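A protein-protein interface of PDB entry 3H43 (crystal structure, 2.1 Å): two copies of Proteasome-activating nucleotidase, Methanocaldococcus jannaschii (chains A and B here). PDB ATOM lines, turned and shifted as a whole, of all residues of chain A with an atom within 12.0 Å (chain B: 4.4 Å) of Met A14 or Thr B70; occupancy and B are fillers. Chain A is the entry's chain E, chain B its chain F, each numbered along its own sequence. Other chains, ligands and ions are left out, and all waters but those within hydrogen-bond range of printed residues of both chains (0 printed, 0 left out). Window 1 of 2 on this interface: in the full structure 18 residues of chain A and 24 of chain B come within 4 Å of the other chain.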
ATOM      1  N   ASN A   4      19.158   5.661  10.846  1.00  0.00           N
ATOM      2  CA  ASN A   4      20.320   6.180  11.535  1.00  0.00           C
ATOM      3  C   ASN A   4      20.767   7.516  10.973  1.00  0.00           C
ATOM      4  O   ASN A   4      21.295   8.366  11.699  1.00  0.00           O
ATOM      5  CB  ASN A   4      21.459   5.178  11.457  1.00  0.00           C
ATOM      6  CG  ASN A   4      21.846   4.662  12.807  1.00  0.00           C
ATOM      7  OD1 ASN A   4      21.012   4.109  13.530  1.00  0.00           O
ATOM      8  ND2 ASN A   4      23.111   4.847  13.173  1.00  0.00           N
ATOM      9  N   GLU A   5      20.544   7.712   9.682  1.00  0.00           N
ATOM     10  CA  GLU A   5      20.948   8.956   9.063  1.00  0.00           C
ATOM     11  C   GLU A   5      20.071  10.115   9.475  1.00  0.00           C
ATOM     12  O   GLU A   5      20.522  11.263   9.500  1.00  0.00           O
ATOM     13  CB  GLU A   5      20.979   8.823   7.541  1.00  0.00           C
ATOM     14  CG  GLU A   5      22.253   8.135   7.053  1.00  0.00           C
ATOM     15  CD  GLU A   5      23.516   8.772   7.630  1.00  0.00           C
ATOM     16  OE1 GLU A   5      23.881   9.889   7.196  1.00  0.00           O
ATOM     17  OE2 GLU A   5      24.137   8.157   8.529  1.00  0.00           O
ATOM     18  N   ILE A   6      18.822   9.822   9.814  1.00  0.00           N
ATOM     19  CA  ILE A   6      17.915  10.876  10.232  1.00  0.00           C
ATOM     20  C   ILE A   6      18.368  11.330  11.609  1.00  0.00           C
ATOM     21  O   ILE A   6      18.378  12.523  11.906  1.00  0.00           O
ATOM     22  CB  ILE A   6      16.457  10.378  10.325  1.00  0.00           C
ATOM     23  CG1 ILE A   6      15.986   9.879   8.958  1.00  0.00           C
ATOM     24  CG2 ILE A   6      15.557  11.500  10.819  1.00  0.00           C
ATOM     25  CD1 ILE A   6      14.546   9.393   8.954  1.00  0.00           C
ATOM     26  N   LEU A   7      18.758  10.380  12.448  1.00  0.00           N
ATOM     27  CA  LEU A   7      19.198  10.729  13.789  1.00  0.00           C
ATOM     28  C   LEU A   7      20.547  11.475  13.757  1.00  0.00           C
ATOM     29  O   LEU A   7      20.767  12.408  14.535  1.00  0.00           O
ATOM     30  CB  LEU A   7      19.303   9.472  14.644  1.00  0.00           C
ATOM     31  CG  LEU A   7      17.973   8.753  14.949  1.00  0.00           C
ATOM     32  CD1 LEU A   7      18.265   7.392  15.563  1.00  0.00           C
ATOM     33  CD2 LEU A   7      17.111   9.594  15.899  1.00  0.00           C
ATOM     34  N   ARG A   8      21.437  11.075  12.848  1.00  0.00           N
ATOM     35  CA  ARG A   8      22.744  11.727  12.743  1.00  0.00           C
ATOM     36  C   ARG A   8      22.645  13.152  12.203  1.00  0.00           C
ATOM     37  O   ARG A   8      23.359  14.040  12.665  1.00  0.00           O
ATOM     38  CB  ARG A   8      23.694  10.903  11.868  1.00  0.00           C
ATOM     39  CG  ARG A   8      24.081   9.593  12.503  1.00  0.00           C
ATOM     40  CD  ARG A   8      24.965   8.748  11.606  1.00  0.00           C
ATOM     41  NE  ARG A   8      25.185   7.435  12.205  1.00  0.00           N
ATOM     42  CZ  ARG A   8      25.962   6.491  11.688  1.00  0.00           C
ATOM     43  NH1 ARG A   8      26.605   6.710  10.550  1.00  0.00           N
ATOM     44  NH2 ARG A   8      26.091   5.326  12.311  1.00  0.00           N
ATOM     45  N   ARG A   9      21.767  13.371  11.229  1.00  0.00           N
ATOM     46  CA  ARG A   9      21.593  14.703  10.671  1.00  0.00           C
ATOM     47  C   ARG A   9      21.032  15.638  11.727  1.00  0.00           C
ATOM     48  O   ARG A   9      21.406  16.811  11.793  1.00  0.00           O
ATOM     49  CB  ARG A   9      20.655  14.683   9.460  1.00  0.00           C
ATOM     50  CG  ARG A   9      21.254  14.079   8.192  1.00  0.00           C
ATOM     51  CD  ARG A   9      20.212  14.002   7.081  1.00  0.00           C
ATOM     52  NE  ARG A   9      20.768  13.493   5.827  1.00  0.00           N
ATOM     53  CZ  ARG A   9      20.086  13.406   4.685  1.00  0.00           C
ATOM     54  NH1 ARG A   9      18.815  13.793   4.638  1.00  0.00           N
ATOM     55  NH2 ARG A   9      20.675  12.950   3.585  1.00  0.00           N
ATOM     56  N   GLU A  10      20.137  15.109  12.558  1.00  0.00           N
ATOM     57  CA  GLU A  10      19.506  15.897  13.620  1.00  0.00           C
ATOM     58  C   GLU A  10      20.550  16.272  14.663  1.00  0.00           C
ATOM     59  O   GLU A  10      20.613  17.409  15.131  1.00  0.00           O
ATOM     60  CB  GLU A  10      18.391  15.078  14.275  1.00  0.00           C
ATOM     61  CG  GLU A  10      17.650  15.793  15.386  1.00  0.00           C
ATOM     62  CD  GLU A  10      17.077  17.124  14.941  1.00  0.00           C
ATOM     63  OE1 GLU A  10      16.936  17.334  13.714  1.00  0.00           O
ATOM     64  OE2 GLU A  10      16.758  17.951  15.822  1.00  0.00           O
ATOM     65  N   LEU A  11      21.378  15.304  15.023  1.00  0.00           N
ATOM     66  CA  LEU A  11      22.408  15.551  15.998  1.00  0.00           C
ATOM     67  C   LEU A  11      23.393  16.573  15.403  1.00  0.00           C
ATOM     68  O   LEU A  11      23.778  17.516  16.087  1.00  0.00           O
ATOM     69  CB  LEU A  11      23.096  14.237  16.358  1.00  0.00           C
ATOM     70  CG  LEU A  11      23.972  14.255  17.602  1.00  0.00           C
ATOM     71  CD1 LEU A  11      23.181  14.806  18.808  1.00  0.00           C
ATOM     72  CD2 LEU A  11      24.477  12.829  17.864  1.00  0.00           C
ATOM     73  N   ASP A  12      23.778  16.404  14.133  1.00  0.00           N
ATOM     74  CA  ASP A  12      24.687  17.371  13.492  1.00  0.00           C
ATOM     75  C   ASP A  12      24.096  18.774  13.614  1.00  0.00           C
ATOM     76  O   ASP A  12      24.778  19.704  14.043  1.00  0.00           O
ATOM     77  CB  ASP A  12      24.896  17.079  11.993  1.00  0.00           C
ATOM     78  CG  ASP A  12      25.607  15.758  11.736  1.00  0.00           C
ATOM     79  OD1 ASP A  12      26.379  15.302  12.617  1.00  0.00           O
ATOM     80  OD2 ASP A  12      25.394  15.180  10.644  1.00  0.00           O
ATOM     81  N   ARG A  13      22.830  18.930  13.236  1.00  0.00           N
ATOM     82  CA  ARG A  13      22.187  20.244  13.321  1.00  0.00           C
ATOM     83  C   ARG A  13      22.164  20.851  14.734  1.00  0.00           C
ATOM     84  O   ARG A  13      22.430  22.036  14.906  1.00  0.00           O
ATOM     85  CB  ARG A  13      20.746  20.195  12.793  1.00  0.00           C
ATOM     86  CG  ARG A  13      20.607  19.819  11.331  1.00  0.00           C
ATOM     87  CD  ARG A  13      19.285  20.344  10.743  1.00  0.00           C
ATOM     88  NE  ARG A  13      18.153  20.099  11.630  1.00  0.00           N
ATOM     89  CZ  ARG A  13      17.446  21.055  12.235  1.00  0.00           C
ATOM     90  NH1 ARG A  13      17.747  22.336  12.046  1.00  0.00           N
ATOM     91  NH2 ARG A  13      16.444  20.731  13.047  1.00  0.00           N
ATOM     92  N   MET A  14      21.845  20.044  15.739  1.00  0.00           N
ATOM     93  CA  MET A  14      21.766  20.538  17.110  1.00  0.00           C
ATOM     94  C   MET A  14      23.120  20.871  17.717  1.00  0.00           C
ATOM     95  O   MET A  14      23.197  21.472  18.785  1.00  0.00           O
ATOM     96  CB  MET A  14      21.072  19.508  17.998  1.00  0.00           C
ATOM     97  CG  MET A  14      19.648  19.184  17.560  1.00  0.00           C
ATOM     98  SD  MET A  14      18.882  17.755  18.599  1.00  0.00           S
ATOM     99  CE  MET A  14      18.468  18.708  20.233  1.00  0.00           C
ATOM    100  N   ARG A  15      24.194  20.485  17.050  1.00  0.00           N
ATOM    101  CA  ARG A  15      25.502  20.767  17.604  1.00  0.00           C
ATOM    102  C   ARG A  15      26.273  21.893  16.954  1.00  0.00           C
ATOM    103  O   ARG A  15      27.358  22.236  17.406  1.00  0.00           O
ATOM    104  CB  ARG A  15      26.345  19.507  17.599  1.00  0.00           C
ATOM    105  CG  ARG A  15      25.922  18.527  18.668  1.00  0.00           C
ATOM    106  CD  ARG A  15      26.668  17.246  18.463  1.00  0.00           C
ATOM    107  NE  ARG A  15      26.541  16.347  19.593  1.00  0.00           N
ATOM    108  CZ  ARG A  15      27.026  15.117  19.585  1.00  0.00           C
ATOM    109  NH1 ARG A  15      27.652  14.678  18.503  1.00  0.00           N
ATOM    110  NH2 ARG A  15      26.889  14.337  20.647  1.00  0.00           N
ATOM    111  N   VAL A  16      25.744  22.473  15.891  1.00  0.00           N
ATOM    112  CA  VAL A  16      26.474  23.569  15.285  1.00  0.00           C
ATOM    113  C   VAL A  16      26.413  24.722  16.279  1.00  0.00           C
ATOM    114  O   VAL A  16      25.373  24.963  16.901  1.00  0.00           O
ATOM    115  CB  VAL A  16      25.849  23.998  13.944  1.00  0.00           C
ATOM    116  CG1 VAL A  16      25.925  22.851  12.954  1.00  0.00           C
ATOM    117  CG2 VAL A  16      24.412  24.411  14.150  1.00  0.00           C
ATOM    118  N   PRO A  17      27.527  25.449  16.452  1.00  0.00           N
ATOM    119  CA  PRO A  17      27.501  26.561  17.401  1.00  0.00           C
ATOM    120  C   PRO A  17      26.559  27.676  16.957  1.00  0.00           C
ATOM    121  O   PRO A  17      26.381  27.923  15.771  1.00  0.00           O
ATOM    122  CB  PRO A  17      28.969  27.000  17.462  1.00  0.00           C
ATOM    123  CG  PRO A  17      29.468  26.682  16.074  1.00  0.00           C
ATOM    124  CD  PRO A  17      28.852  25.321  15.815  1.00  0.00           C
ATOM    125  N   PRO A  18      25.918  28.344  17.919  1.00  0.00           N
ATOM    126  CA  PRO A  18      24.990  29.437  17.621  1.00  0.00           C
ATOM    127  C   PRO A  18      25.696  30.735  17.227  1.00  0.00           C
ATOM    128  O   PRO A  18      26.913  30.888  17.412  1.00  0.00           O
ATOM    129  CB  PRO A  18      24.215  29.590  18.929  1.00  0.00           C
ATOM    130  CG  PRO A  18      25.253  29.257  19.959  1.00  0.00           C
ATOM    131  CD  PRO A  18      25.889  28.010  19.356  1.00  0.00           C
ATOM    132  N   LEU A  19      24.926  31.670  16.688  1.00  0.00           N
ATOM    133  CA  LEU A  19      25.473  32.962  16.311  1.00  0.00           C
ATOM    134  C   LEU A  19      24.779  34.032  17.156  1.00  0.00           C
ATOM    135  O   LEU A  19      23.584  33.933  17.450  1.00  0.00           O
ATOM    136  CB  LEU A  19      25.228  33.238  14.822  1.00  0.00           C
ATOM    137  CG  LEU A  19      25.764  32.241  13.774  1.00  0.00           C
ATOM    138  CD1 LEU A  19      25.212  32.636  12.411  1.00  0.00           C
ATOM    139  CD2 LEU A  19      27.301  32.245  13.741  1.00  0.00           C
ATOM    140  N   ILE A  20      25.537  35.044  17.554  1.00  0.00           N
ATOM    141  CA  ILE A  20      24.996  36.153  18.323  1.00  0.00           C
ATOM    142  C   ILE A  20      24.366  37.162  17.349  1.00  0.00           C
ATOM    143  O   ILE A  20      24.936  37.473  16.306  1.00  0.00           O
ATOM    144  CB  ILE A  20      26.112  36.855  19.120  1.00  0.00           C
ATOM    145  CG1 ILE A  20      26.690  35.876  20.146  1.00  0.00           C
ATOM    146  CG2 ILE A  20      25.576  38.140  19.791  1.00  0.00           C
ATOM    147  CD1 ILE A  20      27.934  36.373  20.813  1.00  0.00           C
ATOM    148  N   GLN A  66      30.660  33.661  17.508  1.00  0.00           N
ATOM    149  CA  GLN A  66      30.813  33.684  18.960  1.00  0.00           C
ATOM    150  C   GLN A  66      32.135  34.189  19.536  1.00  0.00           C
ATOM    151  O   GLN A  66      32.139  34.960  20.488  1.00  0.00           O
ATOM    152  CB  GLN A  66      30.549  32.297  19.520  1.00  0.00           C
ATOM    153  CG  GLN A  66      29.273  32.212  20.306  1.00  0.00           C
ATOM    154  CD  GLN A  66      29.093  30.852  20.912  1.00  0.00           C
ATOM    155  OE1 GLN A  66      28.881  29.871  20.203  1.00  0.00           O
ATOM    156  NE2 GLN A  66      29.195  30.776  22.233  1.00  0.00           N
ATOM    157  N   LEU B  11      20.844  12.389  21.601  1.00  0.00           N
ATOM    158  CA  LEU B  11      19.851  13.413  21.318  1.00  0.00           C
ATOM    159  C   LEU B  11      19.146  13.767  22.636  1.00  0.00           C
ATOM    160  O   LEU B  11      18.969  14.949  22.956  1.00  0.00           O
ATOM    161  CB  LEU B  11      18.842  12.908  20.285  1.00  0.00           C
ATOM    162  CG  LEU B  11      19.375  12.841  18.856  1.00  0.00           C
ATOM    163  CD1 LEU B  11      18.335  12.208  17.958  1.00  0.00           C
ATOM    164  CD2 LEU B  11      19.708  14.239  18.374  1.00  0.00           C
ATOM    165  N   MET B  14      20.723  16.049  25.224  1.00  0.00           N
ATOM    166  CA  MET B  14      20.701  17.457  24.891  1.00  0.00           C
ATOM    167  C   MET B  14      19.473  18.187  25.381  1.00  0.00           C
ATOM    168  O   MET B  14      19.428  19.411  25.341  1.00  0.00           O
ATOM    169  CB  MET B  14      20.850  17.636  23.394  1.00  0.00           C
ATOM    170  CG  MET B  14      22.210  17.198  22.926  1.00  0.00           C
ATOM    171  SD  MET B  14      22.621  17.824  21.177  1.00  0.00           S
ATOM    172  CE  MET B  14      23.319  19.577  21.644  1.00  0.00           C
ATOM    173  N   ASN B  46      19.317  26.777  15.940  1.00  0.00           N
ATOM    174  CA  ASN B  46      18.572  25.776  15.203  1.00  0.00           C
ATOM    175  C   ASN B  46      17.408  25.261  16.050  1.00  0.00           C
ATOM    176  O   ASN B  46      17.442  25.296  17.284  1.00  0.00           O
ATOM    177  CB  ASN B  46      19.483  24.610  14.789  1.00  0.00           C
ATOM    178  CG  ASN B  46      20.192  24.863  13.453  1.00  0.00           C
ATOM    179  OD1 ASN B  46      19.634  25.482  12.548  1.00  0.00           O
ATOM    180  ND2 ASN B  46      21.420  24.363  13.321  1.00  0.00           N
ATOM    181  N   SER B  48      15.350  22.040  17.026  1.00  0.00           N
ATOM    182  CA  SER B  48      15.425  20.585  16.950  1.00  0.00           C
ATOM    183  C   SER B  48      14.105  20.009  16.447  1.00  0.00           C
ATOM    184  O   SER B  48      13.051  20.658  16.531  1.00  0.00           O
ATOM    185  CB  SER B  48      15.764  19.976  18.316  1.00  0.00           C
ATOM    186  OG  SER B  48      14.624  19.922  19.149  1.00  0.00           O
ATOM    187  N   PHE B  50      12.548  17.935  17.793  1.00  0.00           N
ATOM    188  CA  PHE B  50      11.729  17.667  18.977  1.00  0.00           C
ATOM    189  C   PHE B  50      10.633  18.732  19.013  1.00  0.00           C
ATOM    190  O   PHE B  50       9.670  18.628  19.772  1.00  0.00           O
ATOM    191  CB  PHE B  50      12.530  17.826  20.279  1.00  0.00           C
ATOM    192  CG  PHE B  50      13.610  16.802  20.491  1.00  0.00           C
ATOM    193  CD1 PHE B  50      13.345  15.440  20.363  1.00  0.00           C
ATOM    194  CD2 PHE B  50      14.882  17.201  20.900  1.00  0.00           C
ATOM    195  CE1 PHE B  50      14.333  14.491  20.645  1.00  0.00           C
ATOM    196  CE2 PHE B  50      15.874  16.263  21.185  1.00  0.00           C
ATOM    197  CZ  PHE B  50      15.600  14.906  21.059  1.00  0.00           C
ATOM    198  N   CYS B  63      12.833  26.182  25.394  1.00  0.00           N
ATOM    199  CA  CYS B  63      13.928  25.665  26.217  1.00  0.00           C
ATOM    200  C   CYS B  63      15.133  25.474  25.316  1.00  0.00           C
ATOM    201  O   CYS B  63      15.034  24.855  24.250  1.00  0.00           O
ATOM    202  CB  CYS B  63      13.524  24.341  26.858  1.00  0.00           C
ATOM    203  SG  CYS B  63      12.045  24.553  27.872  1.00  0.00           S
ATOM    204  N   LEU B  64      16.265  26.008  25.758  1.00  0.00           N
ATOM    205  CA  LEU B  64      17.495  25.951  24.988  1.00  0.00           C
ATOM    206  C   LEU B  64      18.572  25.081  25.629  1.00  0.00           C
ATOM    207  O   LEU B  64      18.848  25.204  26.827  1.00  0.00           O
ATOM    208  CB  LEU B  64      18.055  27.374  24.827  1.00  0.00           C
ATOM    209  CG  LEU B  64      17.086  28.476  24.380  1.00  0.00           C
ATOM    210  CD1 LEU B  64      17.832  29.818  24.292  1.00  0.00           C
ATOM    211  CD2 LEU B  64      16.474  28.109  23.039  1.00  0.00           C
ATOM    212  N   ASN B  65      19.185  24.210  24.834  1.00  0.00           N
ATOM    213  CA  ASN B  65      20.273  23.385  25.342  1.00  0.00           C
ATOM    214  C   ASN B  65      21.315  24.387  25.849  1.00  0.00           C
ATOM    215  O   ASN B  65      21.546  25.428  25.219  1.00  0.00           O
ATOM    216  CB  ASN B  65      20.860  22.525  24.225  1.00  0.00           C
ATOM    217  CG  ASN B  65      22.110  21.785  24.664  1.00  0.00           C
ATOM    218  OD1 ASN B  65      23.241  22.216  24.390  1.00  0.00           O
ATOM    219  ND2 ASN B  65      21.914  20.672  25.369  1.00  0.00           N
ATOM    220  N   THR B  68      24.583  24.579  23.113  1.00  0.00           N
ATOM    221  CA  THR B  68      24.406  25.071  21.753  1.00  0.00           C
ATOM    222  C   THR B  68      23.230  26.027  21.622  1.00  0.00           C
ATOM    223  O   THR B  68      23.046  26.644  20.573  1.00  0.00           O
ATOM    224  CB  THR B  68      24.138  23.908  20.771  1.00  0.00           C
ATOM    225  OG1 THR B  68      22.858  23.317  21.065  1.00  0.00           O
ATOM    226  CG2 THR B  68      25.224  22.846  20.893  1.00  0.00           C
ATOM    227  N   LEU B  69      22.419  26.130  22.669  1.00  0.00           N
ATOM    228  CA  LEU B  69      21.239  26.982  22.632  1.00  0.00           C
ATOM    229  C   LEU B  69      20.230  26.494  21.617  1.00  0.00           C
ATOM    230  O   LEU B  69      19.286  27.214  21.272  1.00  0.00           O
ATOM    231  CB  LEU B  69      21.604  28.429  22.314  1.00  0.00           C
ATOM    232  CG  LEU B  69      22.399  29.116  23.422  1.00  0.00           C
ATOM    233  CD1 LEU B  69      22.774  30.521  23.004  1.00  0.00           C
ATOM    234  CD2 LEU B  69      21.563  29.139  24.685  1.00  0.00           C
ATOM    235  N   THR B  70      20.404  25.277  21.127  1.00  0.00           N
ATOM    236  CA  THR B  70      19.419  24.770  20.191  1.00  0.00           C
ATOM    237  C   THR B  70      18.091  24.641  20.943  1.00  0.00           C
ATOM    238  O   THR B  70      18.074  24.320  22.137  1.00  0.00           O
ATOM    239  CB  THR B  70      19.811  23.391  19.591  1.00  0.00           C
ATOM    240  OG1 THR B  70      18.715  22.896  18.809  1.00  0.00           O
ATOM    241  CG2 THR B  70      20.132  22.379  20.676  1.00  0.00           C
ATOM    242  N   VAL B  71      16.994  24.927  20.243  1.00  0.00           N
ATOM    243  CA  VAL B  71      15.645  24.843  20.796  1.00  0.00           C
ATOM    244  C   VAL B  71      15.252  23.365  20.905  1.00  0.00           C
ATOM    245  O   VAL B  71      15.053  22.695  19.901  1.00  0.00           O
ATOM    246  CB  VAL B  71      14.632  25.581  19.892  1.00  0.00           C
ATOM    247  CG1 VAL B  71      13.201  25.391  20.416  1.00  0.00           C
ATOM    248  CG2 VAL B  71      14.981  27.058  19.834  1.00  0.00           C
ATOM    249  N   VAL B  72      15.150  22.861  22.132  1.00  0.00           N
ATOM    250  CA  VAL B  72      14.812  21.459  22.334  1.00  0.00           C
ATOM    251  C   VAL B  72      13.385  21.287  22.809  1.00  0.00           C
ATOM    252  O   VAL B  72      12.878  20.170  22.859  1.00  0.00           O
ATOM    253  CB  VAL B  72      15.759  20.787  23.342  1.00  0.00           C
ATOM    254  CG1 VAL B  72      17.176  20.791  22.797  1.00  0.00           C
ATOM    255  CG2 VAL B  72      15.713  21.516  24.663  1.00  0.00           C
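The side-chain amide nitrogen (ND2) of Asn B46 sits at hydrogen-bond distance from the backbone carbonyl oxygen (O) of Arg A13, at 3.0 Å.
The backbone carbonyl oxygen (O) of Met A14 lies within hydrogen-bond range of the side-chain hydroxyl (OG1) of Thr B68.
The side-chain carboxylate of Glu A10 lies within salt-bridge range of the guanidinium group of Arg A13.
The backbone carbonyl oxygen of Asn B46 is in hydrogen-bond range of the side-chain hydroxyl of Thr B70, 3.1 Å away.
The side-chain hydroxyl (OG) of Ser B48 lies close to the backbone NH (N) of Phe B50 (3.2 Å).
OG of Ser B48 lies within hydrogen-bond range of O of Val B71.
N of Asn B65 is in hydrogen-bond range of O of Thr B70 (2.9 Å).
OG1 of Thr B68 sits close to N of Thr B70, at 3.1 Å.
Among the printed residues, merely in contact across the chains: Val A16 with Asn B46, Glu A10 with Ser B48, Pro A18 with Thr B68, Met A14 with Met B14, Leu A7 with Leu B11, Leu A11 with Leu B11, Met A14 with Val B72, Met A14 with Ser B48, Met A14 with Leu B11, Met A14 with Phe B50, Met A14 with Thr B70, Leu A11 with Met B14, Arg A15 with Thr B68 and Glu A10 with Leu B11.
Met A14 touches just these residues of chain B: Leu B11, Met B14, Ser B48, Phe B50, Thr B68, Thr B70 and Val B72.
Thr B70 touches just one residue of chain A: Met A14.
Of chain A, only Arg A13 (3.0 Å) and Val A16 (3.1 Å) come within 4 Å of Asn B46.
Ser B48 touches just these residues of chain A: Glu A10 (3.2 Å) and Met A14 (3.5 Å).
No residue of chain A comes within 4 Å of Leu B64.
Of chain A, only Met A14 (3.0 Å), Arg A15 (3.9 Å) and Pro A18 (3.4 Å) come within 4 Å of Thr B68.
No residue of chain A comes within 4 Å of Leu B69.
Of chain A, only Met A14 comes within 4 Å of Val B72.
Of the printed residues of chain B, Arg A13 touches Asn B46 (3.0 Å).
Of the printed residues of chain B, Val A16 touches Asn B46.
Ile A6 touches none of the printed residues of chain B.
The nearest printed residue of chain B that does not touch Leu A11 is Thr B68 (7.3 Å).
Hydrophobic or aromatic side chains of chain B within 4 Å of the printed part of chain A: Leu B11, Met B14, Phe B50 and Val B72.
Of the 18 printed residues of chain A, 8 touch a printed residue of chain B.
Among the printed residues, 16 pairs touch across the chains.
Among the printed residues, no Asp or Glu carboxylate lies within 4 Å of a Lys or Arg side-chain nitrogen of the other chain.
Leu B11 touches its own counterpart, Leu A11.
Leu A11 touches Met B14, and with the chains exchanged Met A14 touches Leu B11.
Met A14 touches its own counterpart, Met B14.
Positions printed for both chains: 11 and 14.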
